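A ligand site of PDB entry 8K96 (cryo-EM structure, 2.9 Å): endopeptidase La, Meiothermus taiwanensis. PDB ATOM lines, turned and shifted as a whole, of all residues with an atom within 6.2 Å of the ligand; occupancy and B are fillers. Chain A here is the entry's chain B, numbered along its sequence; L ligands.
The backbone NH (N) of Ser 582 lies close to an oxygen (O4) of the ligand. The side-chain hydroxyl of Ser 582 is covalently linked to a boron (B1) of the ligand (1.4 Å). A nitrogen (N1) of the ligand lies close to the backbone carbonyl oxygen (O) of Tyr 575, 2.7 Å away. N of Val 504 sits at hydrogen-bond distance from O2 of the ligand, at 3.1 Å. A nitrogen (N3) of the ligand sits at hydrogen-bond distance from the backbone carbonyl oxygen (O) of Val 504, 3.0 Å away. OG of Ser 577 sits close to N2 of the ligand, 3.2 Å away. N of Glu 506 sits close to N1 of the ligand (3.4 Å).
Val 503 touches the ligand. Val 505 touches the ligand. Phe 542 touches the ligand (CE1 to C18, 3.8 Å). Phe 571 touches the ligand. CA of Val 576 touches O1 of the ligand (3.9 Å). Ile 578 touches the ligand. Glu 579 touches the ligand (N to C7, 3.1 Å). Gly 580 touches the ligand. N of Asp 581 touches O4 of the ligand, 3.9 Å away. CB of Ala 583 touches C19 of the ligand (3.6 Å). 15 residues have an atom within 4 Å of the ligand: Val 503, Val 504, Val 505, Glu 506, Phe 542, Phe 571, Tyr 575, Val 576, Ser 577, Ile 578, Glu 579, Gly 580, Asp 581, Ser 582 and Ala 583. The nearest printed residue that does not touch the ligand is Lys 625 (4.1 Å).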
ATOM      1  N   SER A 501      23.377  -1.202  17.976  1.00  0.00           N
ATOM      2  CA  SER A 501      23.161  -2.278  17.029  1.00  0.00           C
ATOM      3  C   SER A 501      23.267  -3.629  17.706  1.00  0.00           C
ATOM      4  O   SER A 501      24.029  -3.813  18.667  1.00  0.00           O
ATOM      5  CB  SER A 501      24.158  -2.187  15.875  1.00  0.00           C
ATOM      6  OG  SER A 501      24.036  -3.309  15.013  1.00  0.00           O
ATOM      7  N   LEU A 502      22.507  -4.594  17.209  1.00  0.00           N
ATOM      8  CA  LEU A 502      22.462  -5.942  17.756  1.00  0.00           C
ATOM      9  C   LEU A 502      23.239  -6.892  16.861  1.00  0.00           C
ATOM     10  O   LEU A 502      23.055  -6.888  15.640  1.00  0.00           O
ATOM     11  CB  LEU A 502      21.017  -6.428  17.913  1.00  0.00           C
ATOM     12  CG  LEU A 502      20.179  -5.645  18.928  1.00  0.00           C
ATOM     13  CD1 LEU A 502      18.794  -6.243  19.058  1.00  0.00           C
ATOM     14  CD2 LEU A 502      20.873  -5.627  20.268  1.00  0.00           C
ATOM     15  N   VAL A 503      24.114  -7.704  17.461  1.00  0.00           N
ATOM     16  CA  VAL A 503      24.927  -8.653  16.722  1.00  0.00           C
ATOM     17  C   VAL A 503      24.767 -10.032  17.351  1.00  0.00           C
ATOM     18  O   VAL A 503      24.380 -10.161  18.516  1.00  0.00           O
ATOM     19  CB  VAL A 503      26.420  -8.249  16.708  1.00  0.00           C
ATOM     20  CG1 VAL A 503      26.603  -6.899  16.046  1.00  0.00           C
ATOM     21  CG2 VAL A 503      27.004  -8.252  18.110  1.00  0.00           C
ATOM     22  N   VAL A 504      25.079 -11.063  16.574  1.00  0.00           N
ATOM     23  CA  VAL A 504      25.124 -12.437  17.063  1.00  0.00           C
ATOM     24  C   VAL A 504      26.544 -12.952  16.855  1.00  0.00           C
ATOM     25  O   VAL A 504      27.106 -12.848  15.754  1.00  0.00           O
ATOM     26  CB  VAL A 504      24.096 -13.318  16.352  1.00  0.00           C
ATOM     27  CG1 VAL A 504      22.691 -12.981  16.831  1.00  0.00           C
ATOM     28  CG2 VAL A 504      24.172 -13.157  14.846  1.00  0.00           C
ATOM     29  N   VAL A 505      27.132 -13.494  17.924  1.00  0.00           N
ATOM     30  CA  VAL A 505      28.547 -13.870  17.885  1.00  0.00           C
ATOM     31  C   VAL A 505      28.748 -15.058  16.956  1.00  0.00           C
ATOM     32  O   VAL A 505      28.000 -16.038  16.987  1.00  0.00           O
ATOM     33  CB  VAL A 505      29.072 -14.149  19.301  1.00  0.00           C
ATOM     34  CG1 VAL A 505      29.106 -12.870  20.111  1.00  0.00           C
ATOM     35  CG2 VAL A 505      28.212 -15.180  19.993  1.00  0.00           C
ATOM     36  N   GLU A 506      29.768 -14.960  16.095  1.00  0.00           N
ATOM     37  CA  GLU A 506      30.061 -16.040  15.159  1.00  0.00           C
ATOM     38  C   GLU A 506      30.607 -17.276  15.857  1.00  0.00           C
ATOM     39  O   GLU A 506      30.348 -18.398  15.405  1.00  0.00           O
ATOM     40  CB  GLU A 506      31.039 -15.555  14.085  1.00  0.00           C
ATOM     41  CG  GLU A 506      31.367 -16.572  13.011  1.00  0.00           C
ATOM     42  CD  GLU A 506      32.319 -16.016  11.968  1.00  0.00           C
ATOM     43  OE1 GLU A 506      32.662 -14.818  12.052  1.00  0.00           O
ATOM     44  OE2 GLU A 506      32.711 -16.782  11.055  1.00  0.00           O
ATOM     45  N   ALA A 507      31.351 -17.091  16.943  1.00  0.00           N
ATOM     46  CA  ALA A 507      31.860 -18.233  17.710  1.00  0.00           C
ATOM     47  C   ALA A 507      30.734 -19.097  18.251  1.00  0.00           C
ATOM     48  O   ALA A 507      30.950 -20.276  18.525  1.00  0.00           O
ATOM     49  CB  ALA A 507      32.755 -17.747  18.842  1.00  0.00           C
ATOM     50  N   PRO A 509      26.676 -18.984  17.136  1.00  0.00           N
ATOM     51  CA  PRO A 509      25.601 -18.225  16.484  1.00  0.00           C
ATOM     52  C   PRO A 509      24.238 -18.449  17.126  1.00  0.00           C
ATOM     53  O   PRO A 509      23.251 -18.708  16.439  1.00  0.00           O
ATOM     54  CB  PRO A 509      25.632 -18.748  15.042  1.00  0.00           C
ATOM     55  CG  PRO A 509      26.163 -20.143  15.173  1.00  0.00           C
ATOM     56  CD  PRO A 509      27.144 -20.115  16.309  1.00  0.00           C
ATOM     57  N   ALA A 515      25.868  -4.038  20.099  1.00  0.00           N
ATOM     58  CA  ALA A 515      27.137  -3.464  19.669  1.00  0.00           C
ATOM     59  C   ALA A 515      26.911  -1.977  19.438  1.00  0.00           C
ATOM     60  O   ALA A 515      26.043  -1.598  18.656  1.00  0.00           O
ATOM     61  CB  ALA A 515      27.660  -4.140  18.397  1.00  0.00           C
ATOM     62  N   LEU A 517      27.148   0.843  17.675  1.00  0.00           N
ATOM     63  CA  LEU A 517      27.500   1.418  16.397  1.00  0.00           C
ATOM     64  C   LEU A 517      27.409   2.934  16.473  1.00  0.00           C
ATOM     65  O   LEU A 517      26.486   3.488  17.088  1.00  0.00           O
ATOM     66  CB  LEU A 517      26.583   0.899  15.290  1.00  0.00           C
ATOM     67  CG  LEU A 517      26.922   1.256  13.838  1.00  0.00           C
ATOM     68  CD1 LEU A 517      26.392   0.201  12.920  1.00  0.00           C
ATOM     69  CD2 LEU A 517      26.353   2.601  13.432  1.00  0.00           C
ATOM     70  N   PHE A 542      28.098  -8.160   3.348  1.00  0.00           N
ATOM     71  CA  PHE A 542      28.200  -6.808   3.881  1.00  0.00           C
ATOM     72  C   PHE A 542      28.606  -5.811   2.811  1.00  0.00           C
ATOM     73  O   PHE A 542      28.339  -4.606   2.961  1.00  0.00           O
ATOM     74  CB  PHE A 542      29.222  -6.778   5.023  1.00  0.00           C
ATOM     75  CG  PHE A 542      29.141  -5.528   5.861  1.00  0.00           C
ATOM     76  CD1 PHE A 542      27.926  -4.988   6.210  1.00  0.00           C
ATOM     77  CD2 PHE A 542      30.302  -4.900   6.297  1.00  0.00           C
ATOM     78  CE1 PHE A 542      27.852  -3.840   6.976  1.00  0.00           C
ATOM     79  CE2 PHE A 542      30.235  -3.762   7.056  1.00  0.00           C
ATOM     80  CZ  PHE A 542      29.011  -3.226   7.401  1.00  0.00           C
ATOM     81  N   PHE A 571      31.677   0.234  14.349  1.00  0.00           N
ATOM     82  CA  PHE A 571      31.418  -0.187  15.717  1.00  0.00           C
ATOM     83  C   PHE A 571      32.619   0.148  16.591  1.00  0.00           C
ATOM     84  O   PHE A 571      33.762   0.137  16.123  1.00  0.00           O
ATOM     85  CB  PHE A 571      31.126  -1.684  15.782  1.00  0.00           C
ATOM     86  CG  PHE A 571      29.915  -2.112  15.003  1.00  0.00           C
ATOM     87  CD1 PHE A 571      28.656  -2.037  15.563  1.00  0.00           C
ATOM     88  CD2 PHE A 571      30.050  -2.576  13.702  1.00  0.00           C
ATOM     89  CE1 PHE A 571      27.547  -2.438  14.849  1.00  0.00           C
ATOM     90  CE2 PHE A 571      28.937  -2.968  12.986  1.00  0.00           C
ATOM     91  CZ  PHE A 571      27.686  -2.899  13.560  1.00  0.00           C
ATOM     92  N   ASN A 574      35.674  -4.714  18.331  1.00  0.00           N
ATOM     93  CA  ASN A 574      36.195  -5.530  17.257  1.00  0.00           C
ATOM     94  C   ASN A 574      35.617  -6.942  17.230  1.00  0.00           C
ATOM     95  O   ASN A 574      36.057  -7.755  16.405  1.00  0.00           O
ATOM     96  CB  ASN A 574      37.729  -5.613  17.349  1.00  0.00           C
ATOM     97  CG  ASN A 574      38.208  -6.225  18.656  1.00  0.00           C
ATOM     98  OD1 ASN A 574      38.210  -7.437  18.817  1.00  0.00           O
ATOM     99  ND2 ASN A 574      38.594  -5.374  19.594  1.00  0.00           N
ATOM    100  N   TYR A 575      34.658  -7.253  18.090  1.00  0.00           N
ATOM    101  CA  TYR A 575      33.988  -8.546  18.053  1.00  0.00           C
ATOM    102  C   TYR A 575      32.819  -8.582  17.077  1.00  0.00           C
ATOM    103  O   TYR A 575      31.934  -9.414  17.231  1.00  0.00           O
ATOM    104  CB  TYR A 575      33.539  -8.961  19.460  1.00  0.00           C
ATOM    105  CG  TYR A 575      32.487  -8.080  20.121  1.00  0.00           C
ATOM    106  CD1 TYR A 575      31.142  -8.189  19.788  1.00  0.00           C
ATOM    107  CD2 TYR A 575      32.836  -7.162  21.095  1.00  0.00           C
ATOM    108  CE1 TYR A 575      30.187  -7.393  20.394  1.00  0.00           C
ATOM    109  CE2 TYR A 575      31.886  -6.363  21.714  1.00  0.00           C
ATOM    110  CZ  TYR A 575      30.567  -6.479  21.350  1.00  0.00           C
ATOM    111  OH  TYR A 575      29.615  -5.693  21.957  1.00  0.00           O
ATOM    112  N   VAL A 576      32.804  -7.690  16.091  1.00  0.00           N
ATOM    113  CA  VAL A 576      31.654  -7.562  15.206  1.00  0.00           C
ATOM    114  C   VAL A 576      32.061  -7.772  13.753  1.00  0.00           C
ATOM    115  O   VAL A 576      31.521  -7.131  12.843  1.00  0.00           O
ATOM    116  CB  VAL A 576      30.977  -6.184  15.383  1.00  0.00           C
ATOM    117  CG1 VAL A 576      30.356  -6.096  16.769  1.00  0.00           C
ATOM    118  CG2 VAL A 576      31.999  -5.078  15.194  1.00  0.00           C
ATOM    119  N   SER A 577      33.023  -8.671  13.512  1.00  0.00           N
ATOM    120  CA  SER A 577      33.414  -9.019  12.154  1.00  0.00           C
ATOM    121  C   SER A 577      32.193  -9.462  11.361  1.00  0.00           C
ATOM    122  O   SER A 577      31.593 -10.499  11.652  1.00  0.00           O
ATOM    123  CB  SER A 577      34.470 -10.115  12.175  1.00  0.00           C
ATOM    124  OG  SER A 577      33.977 -11.296  12.788  1.00  0.00           O
ATOM    125  N   ILE A 578      31.838  -8.679  10.353  1.00  0.00           N
ATOM    126  CA  ILE A 578      30.508  -8.760   9.743  1.00  0.00           C
ATOM    127  C   ILE A 578      30.449  -9.914   8.757  1.00  0.00           C
ATOM    128  O   ILE A 578      31.324 -10.056   7.894  1.00  0.00           O
ATOM    129  CB  ILE A 578      30.128  -7.443   9.070  1.00  0.00           C
ATOM    130  CG1 ILE A 578      30.169  -6.273  10.059  1.00  0.00           C
ATOM    131  CG2 ILE A 578      28.742  -7.561   8.459  1.00  0.00           C
ATOM    132  CD1 ILE A 578      31.466  -5.485  10.039  1.00  0.00           C
ATOM    133  N   GLU A 579      29.405 -10.733   8.875  1.00  0.00           N
ATOM    134  CA  GLU A 579      29.055 -11.759   7.881  1.00  0.00           C
ATOM    135  C   GLU A 579      27.533 -11.783   7.819  1.00  0.00           C
ATOM    136  O   GLU A 579      26.889 -12.503   8.584  1.00  0.00           O
ATOM    137  CB  GLU A 579      29.621 -13.120   8.254  1.00  0.00           C
ATOM    138  CG  GLU A 579      31.133 -13.246   8.163  1.00  0.00           C
ATOM    139  CD  GLU A 579      31.611 -14.670   8.337  1.00  0.00           C
ATOM    140  OE1 GLU A 579      30.757 -15.573   8.451  1.00  0.00           O
ATOM    141  OE2 GLU A 579      32.835 -14.882   8.353  1.00  0.00           O
ATOM    142  N   GLY A 580      26.966 -11.002   6.916  1.00  0.00           N
ATOM    143  CA  GLY A 580      25.525 -10.891   6.766  1.00  0.00           C
ATOM    144  C   GLY A 580      25.067  -9.442   6.796  1.00  0.00           C
ATOM    145  O   GLY A 580      25.834  -8.513   7.035  1.00  0.00           O
ATOM    146  N   ASP A 581      23.764  -9.266   6.539  1.00  0.00           N
ATOM    147  CA  ASP A 581      23.146  -7.951   6.461  1.00  0.00           C
ATOM    148  C   ASP A 581      22.371  -7.588   7.720  1.00  0.00           C
ATOM    149  O   ASP A 581      21.463  -6.758   7.670  1.00  0.00           O
ATOM    150  CB  ASP A 581      22.241  -7.855   5.234  1.00  0.00           C
ATOM    151  CG  ASP A 581      23.010  -7.858   3.942  1.00  0.00           C
ATOM    152  OD1 ASP A 581      24.174  -7.398   3.938  1.00  0.00           O
ATOM    153  OD2 ASP A 581      22.463  -8.326   2.915  1.00  0.00           O
ATOM    154  N   SER A 582      22.714  -8.176   8.870  1.00  0.00           N
ATOM    155  CA  SER A 582      22.127  -7.720  10.120  1.00  0.00           C
ATOM    156  C   SER A 582      22.607  -6.304  10.432  1.00  0.00           C
ATOM    157  O   SER A 582      23.386  -5.702   9.683  1.00  0.00           O
ATOM    158  CB  SER A 582      22.458  -8.691  11.253  1.00  0.00           C
ATOM    159  OG  SER A 582      23.851  -8.755  11.534  1.00  0.00           O
ATOM    160  N   ALA A 583      22.086  -5.757  11.533  1.00  0.00           N
ATOM    161  CA  ALA A 583      22.208  -4.335  11.855  1.00  0.00           C
ATOM    162  C   ALA A 583      21.393  -3.534  10.845  1.00  0.00           C
ATOM    163  O   ALA A 583      20.245  -3.165  11.118  1.00  0.00           O
ATOM    164  CB  ALA A 583      23.661  -3.851  11.898  1.00  0.00           C
ATOM    165  N   GLY A 584      21.981  -3.255   9.676  1.00  0.00           N
ATOM    166  CA  GLY A 584      21.212  -2.705   8.572  1.00  0.00           C
ATOM    167  C   GLY A 584      20.526  -1.402   8.911  1.00  0.00           C
ATOM    168  O   GLY A 584      21.137  -0.329   8.917  1.00  0.00           O
ATOM    169  N   GLU A 587      22.440   0.794  11.001  1.00  0.00           N
ATOM    170  CA  GLU A 587      23.404   1.623  10.304  1.00  0.00           C
ATOM    171  C   GLU A 587      22.722   2.806   9.647  1.00  0.00           C
ATOM    172  O   GLU A 587      23.224   3.939   9.703  1.00  0.00           O
ATOM    173  CB  GLU A 587      24.161   0.805   9.267  1.00  0.00           C
ATOM    174  CG  GLU A 587      24.999  -0.320   9.804  1.00  0.00           C
ATOM    175  CD  GLU A 587      25.271  -1.388   8.772  1.00  0.00           C
ATOM    176  OE1 GLU A 587      24.300  -2.040   8.308  1.00  0.00           O
ATOM    177  OE2 GLU A 587      26.449  -1.582   8.420  1.00  0.00           O
ATOM    178  N   GLY A 620      17.803 -13.197  10.584  1.00  0.00           N
ATOM    179  CA  GLY A 620      17.798 -14.404  11.384  1.00  0.00           C
ATOM    180  C   GLY A 620      18.251 -14.166  12.822  1.00  0.00           C
ATOM    181  O   GLY A 620      18.907 -13.182  13.143  1.00  0.00           O
ATOM    182  N   LYS A 625      19.075 -11.890  19.404  1.00  0.00           N
ATOM    183  CA  LYS A 625      19.415 -10.477  19.536  1.00  0.00           C
ATOM    184  C   LYS A 625      18.569  -9.804  20.605  1.00  0.00           C
ATOM    185  O   LYS A 625      19.075  -9.050  21.444  1.00  0.00           O
ATOM    186  CB  LYS A 625      19.252  -9.772  18.188  1.00  0.00           C
ATOM    187  CG  LYS A 625      20.249 -10.193  17.123  1.00  0.00           C
ATOM    188  CD  LYS A 625      19.856  -9.637  15.767  1.00  0.00           C
ATOM    189  CE  LYS A 625      20.827 -10.089  14.681  1.00  0.00           C
ATOM    190  NZ  LYS A 625      20.209 -10.024  13.339  1.00  0.00           N
HETATM  191  N1  LIG L   1      30.923 -11.934  17.046  1.00  0.00           N
HETATM  192  C1  LIG L   1      30.826 -11.921  15.721  1.00  0.00           C
HETATM  193  C2  LIG L   1      31.849 -12.392  14.908  1.00  0.00           C
HETATM  194  N2  LIG L   1      32.968 -12.908  15.420  1.00  0.00           N
HETATM  195  C3  LIG L   1      33.046 -12.936  16.748  1.00  0.00           C
HETATM  196  C4  LIG L   1      32.045 -12.459  17.560  1.00  0.00           C
HETATM  197  C5  LIG L   1      29.592 -11.337  15.104  1.00  0.00           C
HETATM  198  O1  LIG L   1      28.983 -10.412  15.647  1.00  0.00           O
HETATM  199  N3  LIG L   1      29.229 -11.878  13.940  1.00  0.00           N
HETATM  200  C6  LIG L   1      28.742 -11.105  12.821  1.00  0.00           C
HETATM  201  C7  LIG L   1      28.609 -11.992  11.579  1.00  0.00           C
HETATM  202  C8  LIG L   1      27.798 -13.255  11.797  1.00  0.00           C
HETATM  203  C9  LIG L   1      26.420 -13.249  11.665  1.00  0.00           C
HETATM  204  C10 LIG L   1      25.688 -14.411  11.859  1.00  0.00           C
HETATM  205  C11 LIG L   1      26.327 -15.591  12.183  1.00  0.00           C
HETATM  206  C12 LIG L   1      27.699 -15.609  12.312  1.00  0.00           C
HETATM  207  C13 LIG L   1      28.431 -14.447  12.118  1.00  0.00           C
HETATM  208  C14 LIG L   1      27.444 -10.344  13.053  1.00  0.00           C
HETATM  209  O2  LIG L   1      26.720 -10.574  14.022  1.00  0.00           O
HETATM  210  N4  LIG L   1      27.169  -9.387  12.150  1.00  0.00           N
HETATM  211  C15 LIG L   1      25.867  -8.763  12.014  1.00  0.00           C
HETATM  212  C16 LIG L   1      25.883  -7.664  10.950  1.00  0.00           C
HETATM  213  C17 LIG L   1      26.757  -6.462  11.282  1.00  0.00           C
HETATM  214  C18 LIG L   1      26.573  -5.351  10.252  1.00  0.00           C
HETATM  215  C19 LIG L   1      26.450  -5.947  12.683  1.00  0.00           C
HETATM  216  B1  LIG L   1      24.790  -9.841  11.635  1.00  0.00           B
HETATM  217  O3  LIG L   1      24.318 -10.695  12.586  1.00  0.00           O
HETATM  218  O4  LIG L   1      24.355  -9.958  10.354  1.00  0.00           O
